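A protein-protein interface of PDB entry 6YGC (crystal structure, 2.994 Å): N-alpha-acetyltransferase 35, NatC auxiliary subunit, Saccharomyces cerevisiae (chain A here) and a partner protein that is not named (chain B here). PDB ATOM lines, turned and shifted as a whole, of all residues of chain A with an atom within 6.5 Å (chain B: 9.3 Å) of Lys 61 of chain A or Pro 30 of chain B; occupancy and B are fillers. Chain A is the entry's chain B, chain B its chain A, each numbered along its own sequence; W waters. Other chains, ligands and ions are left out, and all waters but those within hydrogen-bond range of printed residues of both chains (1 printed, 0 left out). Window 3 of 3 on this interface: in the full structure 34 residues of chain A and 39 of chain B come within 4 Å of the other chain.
Printed residues of chain B within 4 Å of Ser 54 of chain A: Ser 32 (2.6 Å).
Of the printed residues of chain B, Glu 56 of chain A touches Lys 20 (3.1 Å), Ser 32 (3.8 Å) and Ile 33 (2.9 Å).
No residue of chain B comes within 4 Å of Ser 60 of chain A.
Lys 61 of chain A touches just these residues of chain B: Leu 27 and Pro 30.
Leu 62 of chain A touches three residues of chain B.
Of the printed residues of chain A, Pro 30 of chain B touches Lys 61 (3.97 Å) and Leu 62 (3.7 Å).
Of the printed residues of chain A, Tyr 31 of chain B touches Leu 62.
Glu 148 of chain B touches none of the printed residues of chain A.
OE2 of Glu 56 of chain A is in salt-bridge range of NZ of Lys 20 of chain B.
The side-chain hydroxyl (OG) of Ser 54 of chain A sits at hydrogen-bond distance from the side-chain hydroxyl (OG) of Ser 32 of chain B (2.6 Å).
N of Ile 33 of chain B lies within hydrogen-bond range of OE2 of Glu 56 of chain A, 2.9 Å away.
Val 35 of chain B touches Thr 52 of chain A (CG2 to O, 3.2 Å).
Glu 56 of chain A touches Ser 32 of chain B (OE2 to C, 3.8 Å).
Leu 27 of chain B touches Lys 61 of chain A.
Lys 61 of chain A touches Pro 30 of chain B (CB to CB, 3.97 Å).
Leu 62 of chain A touches Pro 30 of chain B.
Tyr 31 of chain B touches Leu 62 of chain A.
Leu 62 of chain A touches Ser 32 of chain B.
ND2 of Asn 59 of chain A sits at hydrogen-bond distance from OE1 of Glu 56 of chain A.
N of Lys 61 of chain A lies close to OD1 of Asn 59 of chain A (3.2 Å).
Printed residues of chain A that touch a printed residue of chain B: Thr 52, Ser 54, Glu 56, Lys 61 and Leu 62.
Of the 18 printed residues of chain B, 7 touch a printed residue of chain A.
Hydrophobic or aromatic side chains of chain B that line the printed part of chain A: Leu 27, Pro 30, Ile 33 and Val 35.
Water W1 bridges the backbone carbonyl oxygen of Ser 28 of chain B (2.8 Å) and the side-chain amino group of Lys 61 of chain A (3.5 Å).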
ATOM      1  N   THR A  52     -14.201  17.111   8.916  1.00  0.00           N
ATOM      2  CA  THR A  52     -14.862  18.205   9.614  1.00  0.00           C
ATOM      3  C   THR A  52     -16.349  17.956   9.829  1.00  0.00           C
ATOM      4  O   THR A  52     -16.934  18.539  10.747  1.00  0.00           O
ATOM      5  CB  THR A  52     -14.667  19.518   8.851  1.00  0.00           C
ATOM      6  OG1 THR A  52     -15.134  19.366   7.504  1.00  0.00           O
ATOM      7  CG2 THR A  52     -13.196  19.911   8.835  1.00  0.00           C
ATOM      8  N   SER A  54     -17.567  15.292  10.988  1.00  0.00           N
ATOM      9  CA  SER A  54     -17.628  14.151  11.885  1.00  0.00           C
ATOM     10  C   SER A  54     -18.504  14.455  13.093  1.00  0.00           C
ATOM     11  O   SER A  54     -18.591  15.597  13.556  1.00  0.00           O
ATOM     12  CB  SER A  54     -16.226  13.763  12.354  1.00  0.00           C
ATOM     13  OG  SER A  54     -15.639  14.805  13.112  1.00  0.00           O
ATOM     14  N   GLU A  56     -19.315  13.515  17.207  1.00  0.00           N
ATOM     15  CA  GLU A  56     -18.525  13.215  18.393  1.00  0.00           C
ATOM     16  C   GLU A  56     -19.418  12.572  19.442  1.00  0.00           C
ATOM     17  O   GLU A  56     -20.482  13.107  19.769  1.00  0.00           O
ATOM     18  CB  GLU A  56     -17.866  14.479  18.955  1.00  0.00           C
ATOM     19  CG  GLU A  56     -16.532  14.220  19.633  1.00  0.00           C
ATOM     20  CD  GLU A  56     -15.956  15.460  20.284  1.00  0.00           C
ATOM     21  OE1 GLU A  56     -16.609  16.018  21.192  1.00  0.00           O
ATOM     22  OE2 GLU A  56     -14.854  15.883  19.881  1.00  0.00           O
ATOM     23  N   ASN A  58     -20.729  11.333  23.107  1.00  0.00           N
ATOM     24  CA  ASN A  58     -20.848  11.973  24.416  1.00  0.00           C
ATOM     25  C   ASN A  58     -20.770  13.496  24.334  1.00  0.00           C
ATOM     26  O   ASN A  58     -20.507  14.162  25.340  1.00  0.00           O
ATOM     27  CB  ASN A  58     -19.801  11.431  25.397  1.00  0.00           C
ATOM     28  CG  ASN A  58     -20.013   9.963  25.716  1.00  0.00           C
ATOM     29  OD1 ASN A  58     -19.106   9.145  25.566  1.00  0.00           O
ATOM     30  ND2 ASN A  58     -21.221   9.621  26.150  1.00  0.00           N
ATOM     31  N   ASN A  59     -21.000  14.059  23.149  1.00  0.00           N
ATOM     32  CA  ASN A  59     -21.139  15.499  22.955  1.00  0.00           C
ATOM     33  C   ASN A  59     -22.616  15.770  22.698  1.00  0.00           C
ATOM     34  O   ASN A  59     -23.156  15.348  21.669  1.00  0.00           O
ATOM     35  CB  ASN A  59     -20.269  15.987  21.797  1.00  0.00           C
ATOM     36  CG  ASN A  59     -20.203  17.505  21.707  1.00  0.00           C
ATOM     37  OD1 ASN A  59     -21.119  18.209  22.133  1.00  0.00           O
ATOM     38  ND2 ASN A  59     -19.112  18.014  21.144  1.00  0.00           N
ATOM     39  N   SER A  60     -23.263  16.473  23.631  1.00  0.00           N
ATOM     40  CA  SER A  60     -24.710  16.658  23.560  1.00  0.00           C
ATOM     41  C   SER A  60     -25.127  17.316  22.250  1.00  0.00           C
ATOM     42  O   SER A  60     -26.172  16.980  21.682  1.00  0.00           O
ATOM     43  CB  SER A  60     -25.190  17.486  24.751  1.00  0.00           C
ATOM     44  OG  SER A  60     -24.799  16.892  25.977  1.00  0.00           O
ATOM     45  N   LYS A  61     -24.317  18.248  21.749  1.00  0.00           N
ATOM     46  CA  LYS A  61     -24.638  18.959  20.521  1.00  0.00           C
ATOM     47  C   LYS A  61     -24.339  18.151  19.265  1.00  0.00           C
ATOM     48  O   LYS A  61     -24.794  18.537  18.182  1.00  0.00           O
ATOM     49  CB  LYS A  61     -23.873  20.286  20.474  1.00  0.00           C
ATOM     50  CG  LYS A  61     -23.992  21.108  21.750  1.00  0.00           C
ATOM     51  CD  LYS A  61     -23.139  22.368  21.695  1.00  0.00           C
ATOM     52  CE  LYS A  61     -23.669  23.355  20.669  1.00  0.00           C
ATOM     53  NZ  LYS A  61     -22.893  24.627  20.672  1.00  0.00           N
ATOM     54  N   LEU A  62     -23.604  17.043  19.377  1.00  0.00           N
ATOM     55  CA  LEU A  62     -23.213  16.265  18.211  1.00  0.00           C
ATOM     56  C   LEU A  62     -23.507  14.773  18.321  1.00  0.00           C
ATOM     57  O   LEU A  62     -23.207  14.035  17.376  1.00  0.00           O
ATOM     58  CB  LEU A  62     -21.714  16.450  17.922  1.00  0.00           C
ATOM     59  CG  LEU A  62     -21.269  17.802  17.359  1.00  0.00           C
ATOM     60  CD1 LEU A  62     -19.752  17.874  17.276  1.00  0.00           C
ATOM     61  CD2 LEU A  62     -21.886  18.043  15.994  1.00  0.00           C
ATOM     62  N   ASP A  63     -24.077  14.304  19.428  1.00  0.00           N
ATOM     63  CA  ASP A  63     -24.394  12.891  19.607  1.00  0.00           C
ATOM     64  C   ASP A  63     -25.905  12.714  19.554  1.00  0.00           C
ATOM     65  O   ASP A  63     -26.629  13.266  20.390  1.00  0.00           O
ATOM     66  CB  ASP A  63     -23.836  12.358  20.927  1.00  0.00           C
ATOM     67  CG  ASP A  63     -23.806  10.840  20.981  1.00  0.00           C
ATOM     68  OD1 ASP A  63     -24.562  10.195  20.224  1.00  0.00           O
ATOM     69  OD2 ASP A  63     -23.026  10.289  21.785  1.00  0.00           O
ATOM     70  N   LEU A  66     -27.659  10.797  22.713  1.00  0.00           N
ATOM     71  CA  LEU A  66     -27.857  11.462  23.994  1.00  0.00           C
ATOM     72  C   LEU A  66     -29.133  12.291  24.045  1.00  0.00           C
ATOM     73  O   LEU A  66     -29.327  13.042  25.008  1.00  0.00           O
ATOM     74  CB  LEU A  66     -26.657  12.354  24.318  1.00  0.00           C
ATOM     75  CG  LEU A  66     -25.282  11.693  24.401  1.00  0.00           C
ATOM     76  CD1 LEU A  66     -24.287  12.659  25.021  1.00  0.00           C
ATOM     77  CD2 LEU A  66     -25.343  10.392  25.186  1.00  0.00           C
ATOM     78  N   PRO A 286     -26.020  15.859  13.267  1.00  0.00           N
ATOM     79  CA  PRO A 286     -26.200  16.158  14.691  1.00  0.00           C
ATOM     80  C   PRO A 286     -27.672  16.243  15.051  1.00  0.00           C
ATOM     81  O   PRO A 286     -28.521  16.500  14.182  1.00  0.00           O
ATOM     82  CB  PRO A 286     -25.510  17.521  14.858  1.00  0.00           C
ATOM     83  CG  PRO A 286     -24.589  17.634  13.694  1.00  0.00           C
ATOM     84  CD  PRO A 286     -25.275  16.926  12.576  1.00  0.00           C
ATOM     85  N   PRO A 287     -28.019  16.026  16.318  1.00  0.00           N
ATOM     86  CA  PRO A 287     -29.415  16.187  16.734  1.00  0.00           C
ATOM     87  C   PRO A 287     -29.858  17.634  16.612  1.00  0.00           C
ATOM     88  O   PRO A 287     -29.064  18.567  16.753  1.00  0.00           O
ATOM     89  CB  PRO A 287     -29.406  15.727  18.198  1.00  0.00           C
ATOM     90  CG  PRO A 287     -27.992  15.923  18.641  1.00  0.00           C
ATOM     91  CD  PRO A 287     -27.150  15.625  17.437  1.00  0.00           C
ATOM     92  N   LYS B  20     -10.388  24.950  22.456  1.00  0.00           N
ATOM     93  CA  LYS B  20     -11.680  24.338  22.164  1.00  0.00           C
ATOM     94  C   LYS B  20     -12.716  24.716  23.214  1.00  0.00           C
ATOM     95  O   LYS B  20     -13.886  24.951  22.886  1.00  0.00           O
ATOM     96  CB  LYS B  20     -11.544  22.817  22.079  1.00  0.00           C
ATOM     97  CG  LYS B  20     -12.887  22.097  22.074  1.00  0.00           C
ATOM     98  CD  LYS B  20     -12.761  20.606  21.819  1.00  0.00           C
ATOM     99  CE  LYS B  20     -14.140  19.961  21.784  1.00  0.00           C
ATOM    100  NZ  LYS B  20     -14.095  18.520  21.419  1.00  0.00           N
ATOM    101  N   ILE B  23     -13.834  28.356  22.288  1.00  0.00           N
ATOM    102  CA  ILE B  23     -14.550  28.468  21.018  1.00  0.00           C
ATOM    103  C   ILE B  23     -15.930  27.836  21.123  1.00  0.00           C
ATOM    104  O   ILE B  23     -16.917  28.377  20.612  1.00  0.00           O
ATOM    105  CB  ILE B  23     -13.736  27.832  19.877  1.00  0.00           C
ATOM    106  CG1 ILE B  23     -12.400  28.547  19.700  1.00  0.00           C
ATOM    107  CG2 ILE B  23     -14.525  27.876  18.574  1.00  0.00           C
ATOM    108  CD1 ILE B  23     -12.525  29.925  19.090  1.00  0.00           C
ATOM    109  N   ASP B  24     -16.024  26.684  21.794  1.00  0.00           N
ATOM    110  CA  ASP B  24     -17.276  25.934  21.824  1.00  0.00           C
ATOM    111  C   ASP B  24     -18.383  26.676  22.562  1.00  0.00           C
ATOM    112  O   ASP B  24     -19.565  26.471  22.264  1.00  0.00           O
ATOM    113  CB  ASP B  24     -17.052  24.562  22.453  1.00  0.00           C
ATOM    114  CG  ASP B  24     -16.491  23.558  21.466  1.00  0.00           C
ATOM    115  OD1 ASP B  24     -16.208  23.950  20.311  1.00  0.00           O
ATOM    116  OD2 ASP B  24     -16.342  22.376  21.840  1.00  0.00           O
ATOM    117  N   ALA B  25     -18.032  27.531  23.522  1.00  0.00           N
ATOM    118  CA  ALA B  25     -19.059  28.263  24.250  1.00  0.00           C
ATOM    119  C   ALA B  25     -19.714  29.324  23.379  1.00  0.00           C
ATOM    120  O   ALA B  25     -20.914  29.587  23.518  1.00  0.00           O
ATOM    121  CB  ALA B  25     -18.462  28.898  25.504  1.00  0.00           C
ATOM    122  N   ASP B  26     -18.957  29.921  22.460  1.00  0.00           N
ATOM    123  CA  ASP B  26     -19.417  31.071  21.695  1.00  0.00           C
ATOM    124  C   ASP B  26     -19.785  30.738  20.252  1.00  0.00           C
ATOM    125  O   ASP B  26     -20.051  31.656  19.470  1.00  0.00           O
ATOM    126  CB  ASP B  26     -18.353  32.168  21.724  1.00  0.00           C
ATOM    127  CG  ASP B  26     -18.123  32.722  23.119  1.00  0.00           C
ATOM    128  OD1 ASP B  26     -19.108  33.134  23.769  1.00  0.00           O
ATOM    129  OD2 ASP B  26     -16.957  32.734  23.570  1.00  0.00           O
ATOM    130  N   LEU B  27     -19.812  29.464  19.873  1.00  0.00           N
ATOM    131  CA  LEU B  27     -20.169  29.091  18.513  1.00  0.00           C
ATOM    132  C   LEU B  27     -21.614  28.613  18.439  1.00  0.00           C
ATOM    133  O   LEU B  27     -22.156  28.052  19.395  1.00  0.00           O
ATOM    134  CB  LEU B  27     -19.231  28.008  17.962  1.00  0.00           C
ATOM    135  CG  LEU B  27     -18.857  26.774  18.793  1.00  0.00           C
ATOM    136  CD1 LEU B  27     -20.008  25.795  19.011  1.00  0.00           C
ATOM    137  CD2 LEU B  27     -17.674  26.064  18.157  1.00  0.00           C
ATOM    138  N   SER B  28     -22.240  28.864  17.289  1.00  0.00           N
ATOM    139  CA  SER B  28     -23.529  28.253  16.993  1.00  0.00           C
ATOM    140  C   SER B  28     -23.339  26.886  16.346  1.00  0.00           C
ATOM    141  O   SER B  28     -23.987  25.910  16.738  1.00  0.00           O
ATOM    142  CB  SER B  28     -24.353  29.173  16.090  1.00  0.00           C
ATOM    143  OG  SER B  28     -23.745  29.311  14.818  1.00  0.00           O
ATOM    144  N   GLU B  29     -22.437  26.797  15.370  1.00  0.00           N
ATOM    145  CA  GLU B  29     -22.123  25.524  14.736  1.00  0.00           C
ATOM    146  C   GLU B  29     -21.154  24.747  15.616  1.00  0.00           C
ATOM    147  O   GLU B  29     -20.032  25.210  15.845  1.00  0.00           O
ATOM    148  CB  GLU B  29     -21.510  25.742  13.361  1.00  0.00           C
ATOM    149  CG  GLU B  29     -22.070  26.949  12.639  1.00  0.00           C
ATOM    150  CD  GLU B  29     -23.542  26.804  12.318  1.00  0.00           C
ATOM    151  OE1 GLU B  29     -23.923  25.775  11.724  1.00  0.00           O
ATOM    152  OE2 GLU B  29     -24.321  27.714  12.663  1.00  0.00           O
ATOM    153  N   PRO B  30     -21.540  23.585  16.125  1.00  0.00           N
ATOM    154  CA  PRO B  30     -20.637  22.805  16.973  1.00  0.00           C
ATOM    155  C   PRO B  30     -19.538  22.140  16.161  1.00  0.00           C
ATOM    156  O   PRO B  30     -19.744  21.706  15.026  1.00  0.00           O
ATOM    157  CB  PRO B  30     -21.566  21.758  17.598  1.00  0.00           C
ATOM    158  CG  PRO B  30     -22.650  21.588  16.583  1.00  0.00           C
ATOM    159  CD  PRO B  30     -22.847  22.930  15.940  1.00  0.00           C
ATOM    160  N   TYR B  31     -18.358  22.053  16.772  1.00  0.00           N
ATOM    161  CA  TYR B  31     -17.174  21.498  16.131  1.00  0.00           C
ATOM    162  C   TYR B  31     -16.722  20.248  16.871  1.00  0.00           C
ATOM    163  O   TYR B  31     -16.602  20.258  18.100  1.00  0.00           O
ATOM    164  CB  TYR B  31     -16.030  22.518  16.096  1.00  0.00           C
ATOM    165  CG  TYR B  31     -16.320  23.768  15.299  1.00  0.00           C
ATOM    166  CD1 TYR B  31     -17.273  23.769  14.290  1.00  0.00           C
ATOM    167  CD2 TYR B  31     -15.632  24.947  15.553  1.00  0.00           C
ATOM    168  CE1 TYR B  31     -17.537  24.911  13.561  1.00  0.00           C
ATOM    169  CE2 TYR B  31     -15.891  26.093  14.831  1.00  0.00           C
ATOM    170  CZ  TYR B  31     -16.842  26.070  13.836  1.00  0.00           C
ATOM    171  OH  TYR B  31     -17.096  27.213  13.117  1.00  0.00           O
ATOM    172  N   SER B  32     -16.471  19.178  16.121  1.00  0.00           N
ATOM    173  CA  SER B  32     -15.860  17.993  16.696  1.00  0.00           C
ATOM    174  C   SER B  32     -14.370  18.237  16.919  1.00  0.00           C
ATOM    175  O   SER B  32     -13.812  19.256  16.505  1.00  0.00           O
ATOM    176  CB  SER B  32     -16.081  16.781  15.792  1.00  0.00           C
ATOM    177  OG  SER B  32     -15.519  16.999  14.510  1.00  0.00           O
ATOM    178  N   ILE B  33     -13.719  17.279  17.582  1.00  0.00           N
ATOM    179  CA  ILE B  33     -12.311  17.464  17.917  1.00  0.00           C
ATOM    180  C   ILE B  33     -11.439  17.416  16.667  1.00  0.00           C
ATOM    181  O   ILE B  33     -10.377  18.049  16.619  1.00  0.00           O
ATOM    182  CB  ILE B  33     -11.868  16.424  18.967  1.00  0.00           C
ATOM    183  CG1 ILE B  33     -10.459  16.742  19.474  1.00  0.00           C
ATOM    184  CG2 ILE B  33     -11.939  15.013  18.399  1.00  0.00           C
ATOM    185  CD1 ILE B  33      -9.998  15.855  20.607  1.00  0.00           C
ATOM    186  N   VAL B  35     -12.323  18.687  13.816  1.00  0.00           N
ATOM    187  CA  VAL B  35     -12.400  20.004  13.197  1.00  0.00           C
ATOM    188  C   VAL B  35     -11.240  20.869  13.672  1.00  0.00           C
ATOM    189  O   VAL B  35     -10.624  21.597  12.883  1.00  0.00           O
ATOM    190  CB  VAL B  35     -13.757  20.663  13.505  1.00  0.00           C
ATOM    191  CG1 VAL B  35     -13.781  22.101  13.008  1.00  0.00           C
ATOM    192  CG2 VAL B  35     -14.890  19.866  12.884  1.00  0.00           C
ATOM    193  N   TYR B  36     -10.915  20.790  14.965  1.00  0.00           N
ATOM    194  CA  TYR B  36      -9.799  21.562  15.500  1.00  0.00           C
ATOM    195  C   TYR B  36      -8.463  21.012  15.019  1.00  0.00           C
ATOM    196  O   TYR B  36      -7.552  21.779  14.691  1.00  0.00           O
ATOM    197  CB  TYR B  36      -9.852  21.574  17.028  1.00  0.00           C
ATOM    198  CG  TYR B  36     -11.034  22.320  17.601  1.00  0.00           C
ATOM    199  CD1 TYR B  36     -11.001  23.700  17.754  1.00  0.00           C
ATOM    200  CD2 TYR B  36     -12.181  21.643  17.997  1.00  0.00           C
ATOM    201  CE1 TYR B  36     -12.079  24.388  18.281  1.00  0.00           C
ATOM    202  CE2 TYR B  36     -13.265  22.322  18.525  1.00  0.00           C
ATOM    203  CZ  TYR B  36     -13.207  23.694  18.665  1.00  0.00           C
ATOM    204  OH  TYR B  36     -14.281  24.376  19.189  1.00  0.00           O
ATOM    205  N   MET B  83     -12.043  30.629  12.893  1.00  0.00           N
ATOM    206  CA  MET B  83     -12.534  30.767  14.257  1.00  0.00           C
ATOM    207  C   MET B  83     -11.913  31.987  14.916  1.00  0.00           C
ATOM    208  O   MET B  83     -10.702  32.206  14.815  1.00  0.00           O
ATOM    209  CB  MET B  83     -12.230  29.508  15.076  1.00  0.00           C
ATOM    210  CG  MET B  83     -13.106  28.317  14.722  1.00  0.00           C
ATOM    211  SD  MET B  83     -12.422  26.743  15.274  1.00  0.00           S
ATOM    212  CE  MET B  83     -11.210  26.434  13.995  1.00  0.00           C
ATOM    213  N   TYR B 145     -26.244  29.811   7.664  1.00  0.00           N
ATOM    214  CA  TYR B 145     -26.246  29.317   9.033  1.00  0.00           C
ATOM    215  C   TYR B 145     -27.631  28.862   9.479  1.00  0.00           C
ATOM    216  O   TYR B 145     -27.920  28.864  10.680  1.00  0.00           O
ATOM    217  CB  TYR B 145     -25.705  30.385   9.984  1.00  0.00           C
ATOM    218  CG  TYR B 145     -24.295  30.833   9.661  1.00  0.00           C
ATOM    219  CD1 TYR B 145     -23.201  30.043   9.992  1.00  0.00           C
ATOM    220  CD2 TYR B 145     -24.060  32.047   9.032  1.00  0.00           C
ATOM    221  CE1 TYR B 145     -21.912  30.449   9.699  1.00  0.00           C
ATOM    222  CE2 TYR B 145     -22.775  32.462   8.740  1.00  0.00           C
ATOM    223  CZ  TYR B 145     -21.706  31.658   9.072  1.00  0.00           C
ATOM    224  OH  TYR B 145     -20.426  32.066   8.779  1.00  0.00           O
ATOM    225  N   LEU B 146     -28.489  28.485   8.532  1.00  0.00           N
ATOM    226  CA  LEU B 146     -29.827  27.941   8.801  1.00  0.00           C
ATOM    227  C   LEU B 146     -30.639  29.016   9.521  1.00  0.00           C
ATOM    228  O   LEU B 146     -30.635  30.176   9.079  1.00  0.00           O
ATOM    229  CB  LEU B 146     -29.687  26.614   9.538  1.00  0.00           C
ATOM    230  CG  LEU B 146     -29.044  25.486   8.730  1.00  0.00           C
ATOM    231  CD1 LEU B 146     -28.285  24.533   9.639  1.00  0.00           C
ATOM    232  CD2 LEU B 146     -30.102  24.738   7.932  1.00  0.00           C
ATOM    233  N   GLU B 148     -30.086  30.762  11.943  1.00  0.00           N
ATOM    234  CA  GLU B 148     -29.325  31.887  12.474  1.00  0.00           C
ATOM    235  C   GLU B 148     -29.450  33.106  11.569  1.00  0.00           C
ATOM    236  O   GLU B 148     -29.463  34.246  12.048  1.00  0.00           O
ATOM    237  CB  GLU B 148     -27.859  31.495  12.650  1.00  0.00           C
ATOM    238  CG  GLU B 148     -27.621  30.416  13.697  1.00  0.00           C
ATOM    239  CD  GLU B 148     -27.735  30.946  15.114  1.00  0.00           C
ATOM    240  OE1 GLU B 148     -26.706  31.368  15.681  1.00  0.00           O
ATOM    241  OE2 GLU B 148     -28.858  30.950  15.658  1.00  0.00           O
HETATM  242  O   HOH W   1     -25.720  24.930  18.655  1.00  0.00           O
